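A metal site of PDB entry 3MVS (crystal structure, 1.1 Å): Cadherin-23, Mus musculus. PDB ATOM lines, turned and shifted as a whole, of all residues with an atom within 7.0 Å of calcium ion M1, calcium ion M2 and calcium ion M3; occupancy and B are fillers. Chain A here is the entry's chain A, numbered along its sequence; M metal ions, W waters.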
ATOM      1  N   GLU A  21      -3.859  20.061  15.521  1.00  0.00           N
ATOM      2  CA  GLU A  21      -3.035  19.464  14.482  1.00  0.00           C
ATOM      3  C   GLU A  21      -3.678  18.246  13.814  1.00  0.00           C
ATOM      4  O   GLU A  21      -3.214  17.832  12.757  1.00  0.00           O
ATOM      5  CB  GLU A  21      -1.643  19.092  14.998  1.00  0.00           C
ATOM      6  CG  GLU A  21      -1.637  17.926  15.992  1.00  0.00           C
ATOM      7  CD  GLU A  21      -0.250  17.483  16.428  1.00  0.00           C
ATOM      8  OE1 GLU A  21       0.691  17.635  15.625  1.00  0.00           O
ATOM      9  OE2 GLU A  21      -0.123  16.937  17.546  1.00  0.00           O
ATOM     10  N   LEU A  70      -0.986  20.441   9.544  1.00  0.00           N
ATOM     11  CA  LEU A  70      -0.308  21.142  10.622  1.00  0.00           C
ATOM     12  C   LEU A  70       0.396  20.095  11.468  1.00  0.00           C
ATOM     13  O   LEU A  70      -0.032  18.945  11.507  1.00  0.00           O
ATOM     14  CB  LEU A  70      -1.313  21.889  11.495  1.00  0.00           C
ATOM     15  CG  LEU A  70      -2.140  22.938  10.762  1.00  0.00           C
ATOM     16  CD1 LEU A  70      -3.211  23.462  11.692  1.00  0.00           C
ATOM     17  CD2 LEU A  70      -1.269  24.055  10.238  1.00  0.00           C
ATOM     18  N   ASP A  71       1.495  20.478  12.098  1.00  0.00           N
ATOM     19  CA  ASP A  71       2.223  19.534  12.933  1.00  0.00           C
ATOM     20  C   ASP A  71       2.767  20.287  14.115  1.00  0.00           C
ATOM     21  O   ASP A  71       3.719  21.045  13.984  1.00  0.00           O
ATOM     22  CB  ASP A  71       3.341  18.853  12.149  1.00  0.00           C
ATOM     23  CG  ASP A  71       4.140  17.879  12.993  1.00  0.00           C
ATOM     24  OD1 ASP A  71       3.675  17.484  14.083  1.00  0.00           O
ATOM     25  OD2 ASP A  71       5.255  17.483  12.559  1.00  0.00           O
ATOM     26  N   ARG A  72       2.162  20.064  15.276  1.00  0.00           N
ATOM     27  CA  ARG A  72       2.574  20.726  16.502  1.00  0.00           C
ATOM     28  C   ARG A  72       4.037  20.468  16.825  1.00  0.00           C
ATOM     29  O   ARG A  72       4.740  21.333  17.357  1.00  0.00           O
ATOM     30  CB  ARG A  72       1.683  20.282  17.664  1.00  0.00           C
ATOM     31  CG  ARG A  72       1.577  21.238  18.856  1.00  0.00           C
ATOM     32  CD  ARG A  72       2.748  21.211  19.831  1.00  0.00           C
ATOM     33  NE  ARG A  72       3.206  19.847  20.060  1.00  0.00           N
ATOM     34  CZ  ARG A  72       4.387  19.566  20.619  1.00  0.00           C
ATOM     35  NH1 ARG A  72       5.177  20.557  21.015  1.00  0.00           N
ATOM     36  NH2 ARG A  72       4.762  18.302  20.798  1.00  0.00           N
ATOM     37  N   GLU A  73       4.503  19.276  16.459  1.00  0.00           N
ATOM     38  CA  GLU A  73       5.902  18.868  16.712  1.00  0.00           C
ATOM     39  C   GLU A  73       6.926  19.568  15.816  1.00  0.00           C
ATOM     40  O   GLU A  73       8.134  19.477  16.078  1.00  0.00           O
ATOM     41  CB  GLU A  73       6.052  17.346  16.570  1.00  0.00           C
ATOM     42  CG  GLU A  73       5.583  16.506  17.747  1.00  0.00           C
ATOM     43  CD  GLU A  73       4.065  16.446  17.910  1.00  0.00           C
ATOM     44  OE1 GLU A  73       3.298  16.246  16.940  1.00  0.00           O
ATOM     45  OE2 GLU A  73       3.616  16.578  19.054  1.00  0.00           O
ATOM     46  N   THR A  74       6.464  20.249  14.768  1.00  0.00           N
ATOM     47  CA  THR A  74       7.338  20.999  13.855  1.00  0.00           C
ATOM     48  C   THR A  74       7.227  22.494  14.111  1.00  0.00           C
ATOM     49  O   THR A  74       8.241  23.186  14.246  1.00  0.00           O
ATOM     50  CB  THR A  74       7.015  20.696  12.371  1.00  0.00           C
ATOM     51  OG1 THR A  74       7.249  19.319  12.093  1.00  0.00           O
ATOM     52  CG2 THR A  74       7.855  21.553  11.434  1.00  0.00           C
ATOM     53  N   GLY A 100      -2.769  23.158  18.073  1.00  0.00           N
ATOM     54  CA  GLY A 100      -3.050  22.363  19.263  1.00  0.00           C
ATOM     55  C   GLY A 100      -2.459  20.972  19.135  1.00  0.00           C
ATOM     56  O   GLY A 100      -2.533  20.343  18.085  1.00  0.00           O
ATOM     57  N   ASP A 101      -1.883  20.479  20.226  1.00  0.00           N
ATOM     58  CA  ASP A 101      -1.282  19.148  20.220  1.00  0.00           C
ATOM     59  C   ASP A 101      -2.348  18.081  20.353  1.00  0.00           C
ATOM     60  O   ASP A 101      -3.287  18.222  21.126  1.00  0.00           O
ATOM     61  CB  ASP A 101      -0.293  19.013  21.370  1.00  0.00           C
ATOM     62  CG  ASP A 101       0.523  17.723  21.296  1.00  0.00           C
ATOM     63  OD1 ASP A 101       1.148  17.482  20.256  1.00  0.00           O
ATOM     64  OD2 ASP A 101       0.576  16.957  22.285  1.00  0.00           O
ATOM     65  N   VAL A 102      -2.144  16.980  19.637  1.00  0.00           N
ATOM     66  CA  VAL A 102      -2.849  15.727  19.955  1.00  0.00           C
ATOM     67  C   VAL A 102      -1.805  14.636  20.118  1.00  0.00           C
ATOM     68  O   VAL A 102      -0.637  14.802  19.736  1.00  0.00           O
ATOM     69  CB  VAL A 102      -3.920  15.314  18.898  1.00  0.00           C
ATOM     70  CG1 VAL A 102      -4.892  16.447  18.648  1.00  0.00           C
ATOM     71  CG2 VAL A 102      -3.267  14.849  17.615  1.00  0.00           C
ATOM     72  N   ASN A 103      -2.213  13.491  20.655  1.00  0.00           N
ATOM     73  CA  ASN A 103      -1.289  12.374  20.761  1.00  0.00           C
ATOM     74  C   ASN A 103      -1.243  11.665  19.424  1.00  0.00           C
ATOM     75  O   ASN A 103      -2.112  10.844  19.121  1.00  0.00           O
ATOM     76  CB  ASN A 103      -1.715  11.390  21.845  1.00  0.00           C
ATOM     77  CG  ASN A 103      -0.642  10.372  22.101  1.00  0.00           C
ATOM     78  OD1 ASN A 103       0.509  10.740  22.222  1.00  0.00           O
ATOM     79  ND2 ASN A 103      -1.009   9.109  22.177  1.00  0.00           N
ATOM     80  N   ASP A 104      -0.242  11.987  18.619  1.00  0.00           N
ATOM     81  CA  ASP A 104      -0.127  11.429  17.266  1.00  0.00           C
ATOM     82  C   ASP A 104       1.223  10.792  16.964  1.00  0.00           C
ATOM     83  O   ASP A 104       1.506  10.425  15.826  1.00  0.00           O
ATOM     84  CB  ASP A 104      -0.533  12.451  16.181  1.00  0.00           C
ATOM     85  CG  ASP A 104       0.328  13.720  16.159  1.00  0.00           C
ATOM     86  OD1 ASP A 104       1.087  14.001  17.108  1.00  0.00           O
ATOM     87  OD2 ASP A 104       0.272  14.466  15.150  1.00  0.00           O
ATOM     88  N   ASN A 105       2.032  10.634  18.004  1.00  0.00           N
ATOM     89  CA  ASN A 105       3.304   9.912  17.885  1.00  0.00           C
ATOM     90  C   ASN A 105       3.299   8.735  18.841  1.00  0.00           C
ATOM     91  O   ASN A 105       2.881   8.851  19.976  1.00  0.00           O
ATOM     92  CB  ASN A 105       4.512  10.788  18.248  1.00  0.00           C
ATOM     93  CG  ASN A 105       4.727  11.904  17.259  1.00  0.00           C
ATOM     94  OD1 ASN A 105       5.541  11.788  16.335  1.00  0.00           O
ATOM     95  ND2 ASN A 105       3.966  12.988  17.416  1.00  0.00           N
ATOM     96  N   ALA A 106       3.743   7.582  18.356  1.00  0.00           N
ATOM     97  CA  ALA A 106       4.068   6.471  19.248  1.00  0.00           C
ATOM     98  C   ALA A 106       5.509   6.641  19.724  1.00  0.00           C
ATOM     99  O   ALA A 106       6.281   7.393  19.126  1.00  0.00           O
ATOM    100  CB  ALA A 106       3.902   5.148  18.497  1.00  0.00           C
ATOM    101  N   PRO A 107       5.906   5.922  20.783  1.00  0.00           N
ATOM    102  CA  PRO A 107       7.301   6.025  21.254  1.00  0.00           C
ATOM    103  C   PRO A 107       8.321   5.505  20.234  1.00  0.00           C
ATOM    104  O   PRO A 107       8.016   4.618  19.442  1.00  0.00           O
ATOM    105  CB  PRO A 107       7.300   5.176  22.535  1.00  0.00           C
ATOM    106  CG  PRO A 107       5.870   5.255  23.003  1.00  0.00           C
ATOM    107  CD  PRO A 107       5.057   5.194  21.751  1.00  0.00           C
ATOM    108  N   ASP A 135       9.109  10.065  23.355  1.00  0.00           N
ATOM    109  CA  ASP A 135       7.864  10.360  22.669  1.00  0.00           C
ATOM    110  C   ASP A 135       7.656  11.875  22.725  1.00  0.00           C
ATOM    111  O   ASP A 135       7.668  12.444  23.817  1.00  0.00           O
ATOM    112  CB  ASP A 135       6.738   9.618  23.389  1.00  0.00           C
ATOM    113  CG  ASP A 135       5.409   9.689  22.672  1.00  0.00           C
ATOM    114  OD1 ASP A 135       5.007  10.772  22.193  1.00  0.00           O
ATOM    115  OD2 ASP A 135       4.696   8.653  22.631  1.00  0.00           O
ATOM    116  N   PRO A 136       7.459  12.543  21.573  1.00  0.00           N
ATOM    117  CA  PRO A 136       7.484  14.020  21.547  1.00  0.00           C
ATOM    118  C   PRO A 136       6.150  14.680  21.843  1.00  0.00           C
ATOM    119  O   PRO A 136       6.092  15.913  21.912  1.00  0.00           O
ATOM    120  CB  PRO A 136       7.873  14.319  20.106  1.00  0.00           C
ATOM    121  CG  PRO A 136       7.231  13.224  19.330  1.00  0.00           C
ATOM    122  CD  PRO A 136       7.448  11.977  20.219  1.00  0.00           C
ATOM    123  N   ASP A 137       5.064  13.923  21.985  1.00  0.00           N
ATOM    124  CA  ASP A 137       3.782  14.530  22.287  1.00  0.00           C
ATOM    125  C   ASP A 137       3.799  15.166  23.659  1.00  0.00           C
ATOM    126  O   ASP A 137       4.609  14.789  24.505  1.00  0.00           O
ATOM    127  CB  ASP A 137       2.642  13.517  22.180  1.00  0.00           C
ATOM    128  CG  ASP A 137       2.470  12.991  20.770  1.00  0.00           C
ATOM    129  OD1 ASP A 137       2.281  13.808  19.842  1.00  0.00           O
ATOM    130  OD2 ASP A 137       2.555  11.764  20.587  1.00  0.00           O
ATOM    131  N   LEU A 138       2.912  16.111  23.891  1.00  0.00           N
ATOM    132  CA  LEU A 138       2.902  16.826  25.144  1.00  0.00           C
ATOM    133  C   LEU A 138       2.182  16.054  26.230  1.00  0.00           C
ATOM    134  O   LEU A 138       1.320  15.203  25.936  1.00  0.00           O
ATOM    135  CB  LEU A 138       2.267  18.216  24.970  1.00  0.00           C
ATOM    136  CG  LEU A 138       2.961  19.105  23.953  1.00  0.00           C
ATOM    137  CD1 LEU A 138       2.301  20.479  23.892  1.00  0.00           C
ATOM    138  CD2 LEU A 138       4.461  19.255  24.274  1.00  0.00           C
ATOM    139  N   ALA A 140       0.706  13.665  29.044  1.00  0.00           N
ATOM    140  CA  ALA A 140       0.633  12.219  29.232  1.00  0.00           C
ATOM    141  C   ALA A 140       0.938  11.454  27.951  1.00  0.00           C
ATOM    142  O   ALA A 140       1.480  10.356  27.999  1.00  0.00           O
ATOM    143  CB  ALA A 140      -0.724  11.822  29.784  1.00  0.00           C
ATOM    144  N   GLY A 141       0.634  12.066  26.803  1.00  0.00           N
ATOM    145  CA  GLY A 141       0.962  11.456  25.531  1.00  0.00           C
ATOM    146  C   GLY A 141       2.442  11.340  25.237  1.00  0.00           C
ATOM    147  O   GLY A 141       2.812  10.639  24.291  1.00  0.00           O
ATOM    148  N   GLY A 142       3.293  12.020  26.021  1.00  0.00           N
ATOM    149  CA  GLY A 142       4.743  11.919  25.872  1.00  0.00           C
ATOM    150  C   GLY A 142       5.406  11.074  26.945  1.00  0.00           C
ATOM    151  O   GLY A 142       6.621  10.918  26.935  1.00  0.00           O
ATOM    152  N   SER A 143       4.587  10.553  27.867  1.00  0.00           N
ATOM    153  CA  SER A 143       5.075   9.724  28.963  1.00  0.00           C
ATOM    154  C   SER A 143       4.982   8.253  28.580  1.00  0.00           C
ATOM    155  O   SER A 143       3.927   7.782  28.180  1.00  0.00           O
ATOM    156  CB  SER A 143       4.242   9.983  30.224  1.00  0.00           C
ATOM    157  OG  SER A 143       4.665   9.166  31.287  1.00  0.00           O
ATOM    158  N   VAL A 144       6.092   7.545  28.723  1.00  0.00           N
ATOM    159  CA  VAL A 144       6.225   6.168  28.225  1.00  0.00           C
ATOM    160  C   VAL A 144       6.298   5.171  29.372  1.00  0.00           C
ATOM    161  O   VAL A 144       7.024   5.386  30.354  1.00  0.00           O
ATOM    162  CB  VAL A 144       7.527   6.068  27.379  1.00  0.00           C
ATOM    163  CG1 VAL A 144       7.729   4.630  26.871  1.00  0.00           C
ATOM    164  CG2 VAL A 144       7.481   7.040  26.203  1.00  0.00           C
ATOM    165  N   ASP A 186       2.550   5.013  25.374  1.00  0.00           N
ATOM    166  CA  ASP A 186       2.373   6.291  26.024  1.00  0.00           C
ATOM    167  C   ASP A 186       1.118   6.307  26.880  1.00  0.00           C
ATOM    168  O   ASP A 186       0.337   5.361  26.899  1.00  0.00           O
ATOM    169  CB  ASP A 186       2.490   7.454  25.013  1.00  0.00           C
ATOM    170  CG  ASP A 186       1.344   7.504  24.029  1.00  0.00           C
ATOM    171  OD1 ASP A 186       0.223   7.092  24.382  1.00  0.00           O
ATOM    172  OD2 ASP A 186       1.548   7.995  22.893  1.00  0.00           O
ATOM    173  N   GLN A 187       0.925   7.389  27.624  1.00  0.00           N
ATOM    174  CA  GLN A 187      -0.089   7.414  28.676  1.00  0.00           C
ATOM    175  C   GLN A 187      -1.260   8.339  28.369  1.00  0.00           C
ATOM    176  O   GLN A 187      -2.004   8.737  29.273  1.00  0.00           O
ATOM    177  CB  GLN A 187       0.560   7.734  30.026  1.00  0.00           C
ATOM    178  CG  GLN A 187       1.617   6.702  30.424  1.00  0.00           C
ATOM    179  CD  GLN A 187       1.044   5.310  30.495  1.00  0.00           C
ATOM    180  OE1 GLN A 187       1.424   4.425  29.728  1.00  0.00           O
ATOM    181  NE2 GLN A 187       0.117   5.107  31.421  1.00  0.00           N
ATOM    182  N   ASP A 188      -1.448   8.677  27.098  1.00  0.00           N
ATOM    183  CA  ASP A 188      -2.612   9.482  26.728  1.00  0.00           C
ATOM    184  C   ASP A 188      -3.892   8.774  27.181  1.00  0.00           C
ATOM    185  O   ASP A 188      -4.040   7.565  27.009  1.00  0.00           O
ATOM    186  CB  ASP A 188      -2.669   9.710  25.220  1.00  0.00           C
ATOM    187  CG  ASP A 188      -3.743  10.700  24.849  1.00  0.00           C
ATOM    188  OD1 ASP A 188      -3.499  11.912  24.960  1.00  0.00           O
ATOM    189  OD2 ASP A 188      -4.848  10.261  24.474  1.00  0.00           O
ATOM    190  N   ARG A 191      -6.386   8.166  23.630  1.00  0.00           N
ATOM    191  CA  ARG A 191      -5.851   7.409  22.507  1.00  0.00           C
ATOM    192  C   ARG A 191      -4.356   7.097  22.675  1.00  0.00           C
ATOM    193  O   ARG A 191      -3.509   7.649  21.954  1.00  0.00           O
ATOM    194  CB  ARG A 191      -6.128   8.120  21.191  1.00  0.00           C
ATOM    195  CG  ARG A 191      -6.554   7.170  20.092  1.00  0.00           C
ATOM    196  N   PRO A 192      -4.037   6.197  23.606  1.00  0.00           N
ATOM    197  CA  PRO A 192      -2.643   5.810  23.786  1.00  0.00           C
ATOM    198  C   PRO A 192      -2.074   5.090  22.557  1.00  0.00           C
ATOM    199  O   PRO A 192      -2.821   4.383  21.857  1.00  0.00           O
ATOM    200  CB  PRO A 192      -2.676   4.898  25.006  1.00  0.00           C
ATOM    201  CG  PRO A 192      -4.071   4.352  25.039  1.00  0.00           C
ATOM    202  CD  PRO A 192      -4.920   5.465  24.532  1.00  0.00           C
ATOM    203  N   LEU A 193      -0.777   5.272  22.323  1.00  0.00           N
ATOM    204  CA  LEU A 193      -0.090   4.688  21.190  1.00  0.00           C
ATOM    205  C   LEU A 193       1.084   3.843  21.641  1.00  0.00           C
ATOM    206  O   LEU A 193       1.757   4.192  22.615  1.00  0.00           O
ATOM    207  CB  LEU A 193       0.375   5.787  20.249  1.00  0.00           C
ATOM    208  CG  LEU A 193      -0.753   6.582  19.586  1.00  0.00           C
ATOM    209  CD1 LEU A 193      -0.147   7.728  18.777  1.00  0.00           C
ATOM    210  CD2 LEU A 193      -1.611   5.731  18.672  1.00  0.00           C
HETATM  211 CA    CA M   1       1.383  15.690  18.826  1.00  0.00          CA
HETATM  212 CA    CA M   2       2.147  15.928  14.941  1.00  0.00          CA
HETATM  213 CA    CA M   3       2.696   9.872  22.083  1.00  0.00          CA
HETATM  214  O   HOH W   1       1.549  15.791  12.700  1.00  0.00           O
HETATM  215  O   HOH W   2       3.659  14.163  14.577  1.00  0.00           O
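Water W1 is bound to calcium ion M2. The side-chain carboxylate (OE1) of Glu 73 binds calcium ion M2 (2.3 Å). Calcium ion M2 is bound by OD1 of Asp 71 (2.3 Å). OE1 of Glu 21 is bound to calcium ion M2. Water W2 is bound to calcium ion M2 (2.4 Å). OD2 of Asp 104 binds calcium ion M2 (2.4 Å). Calcium ion M2 has six donor atoms within binding distance. Slightly farther from calcium ion M2 lies the side-chain carboxylate (OD1) of Asp 104 (3.1 Å).
The side-chain carboxylate (OD2) of Asp 71 is in hydrogen-bond range of the side-chain hydroxyl (OG1) of Thr 74. N of Leu 138 lies within hydrogen-bond range of OD2 of Asp 101, 3.0 Å away. The side-chain amide nitrogen of Asn 103 sits at hydrogen-bond distance from the backbone carbonyl oxygen of Arg 191 (2.9 Å). The backbone NH of Glu 21 sits at hydrogen-bond distance from the backbone carbonyl oxygen of Gly 100 (2.9 Å). O of Asp 137 lies close to N of Gly 142. ND2 of Asn 105 sits close to OE1 of Glu 73. OD1 of Asp 101 sits close to NE of Arg 72, 3.1 Å away. OD1 of Asp 186 is in hydrogen-bond range of N of Leu 193 (2.9 Å).
Calcium ion M3 is bound by O of Gly 141 (2.3 Å), OD2 of Asp 186 (2.3 Å), O of Asn 105 (2.3 Å), OD1 of Asn 103 (2.4 Å), OD2 of Asp 135 (2.4 Å), OD2 of Asp 137 (2.4 Å) and OD1 of Asp 135 (2.5 Å). Calcium ion M3 has seven donor atoms within binding distance.
OD1 of Asp 101 is bound to calcium ion M1 (2.3 Å). Calcium ion M1 is bound by the side-chain carboxylate (OD1) of Asp 137 (2.3 Å). OE2 of Glu 21 is bound to calcium ion M1 (2.3 Å). O of Val 102 is bound to calcium ion M1 (2.4 Å). The side-chain carboxylate (OE2) of Glu 73 binds calcium ion M1. Calcium ion M1 is bound by OD1 of Asp 104 (2.4 Å). OE1 of Glu 73 is bound to calcium ion M1 (2.7 Å).
Of the 29 residues printed, 7 come within 4 Å of calcium ion M1.
Within 4 Å of calcium ion M2: Glu 21, Asp 71, Glu 73 and Asp 104.
Of the 29 residues printed, 6 come within 4 Å of calcium ion M3. The nearest printed residue that does not touch calcium ion M3 is Ala 106 (4.5 Å).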
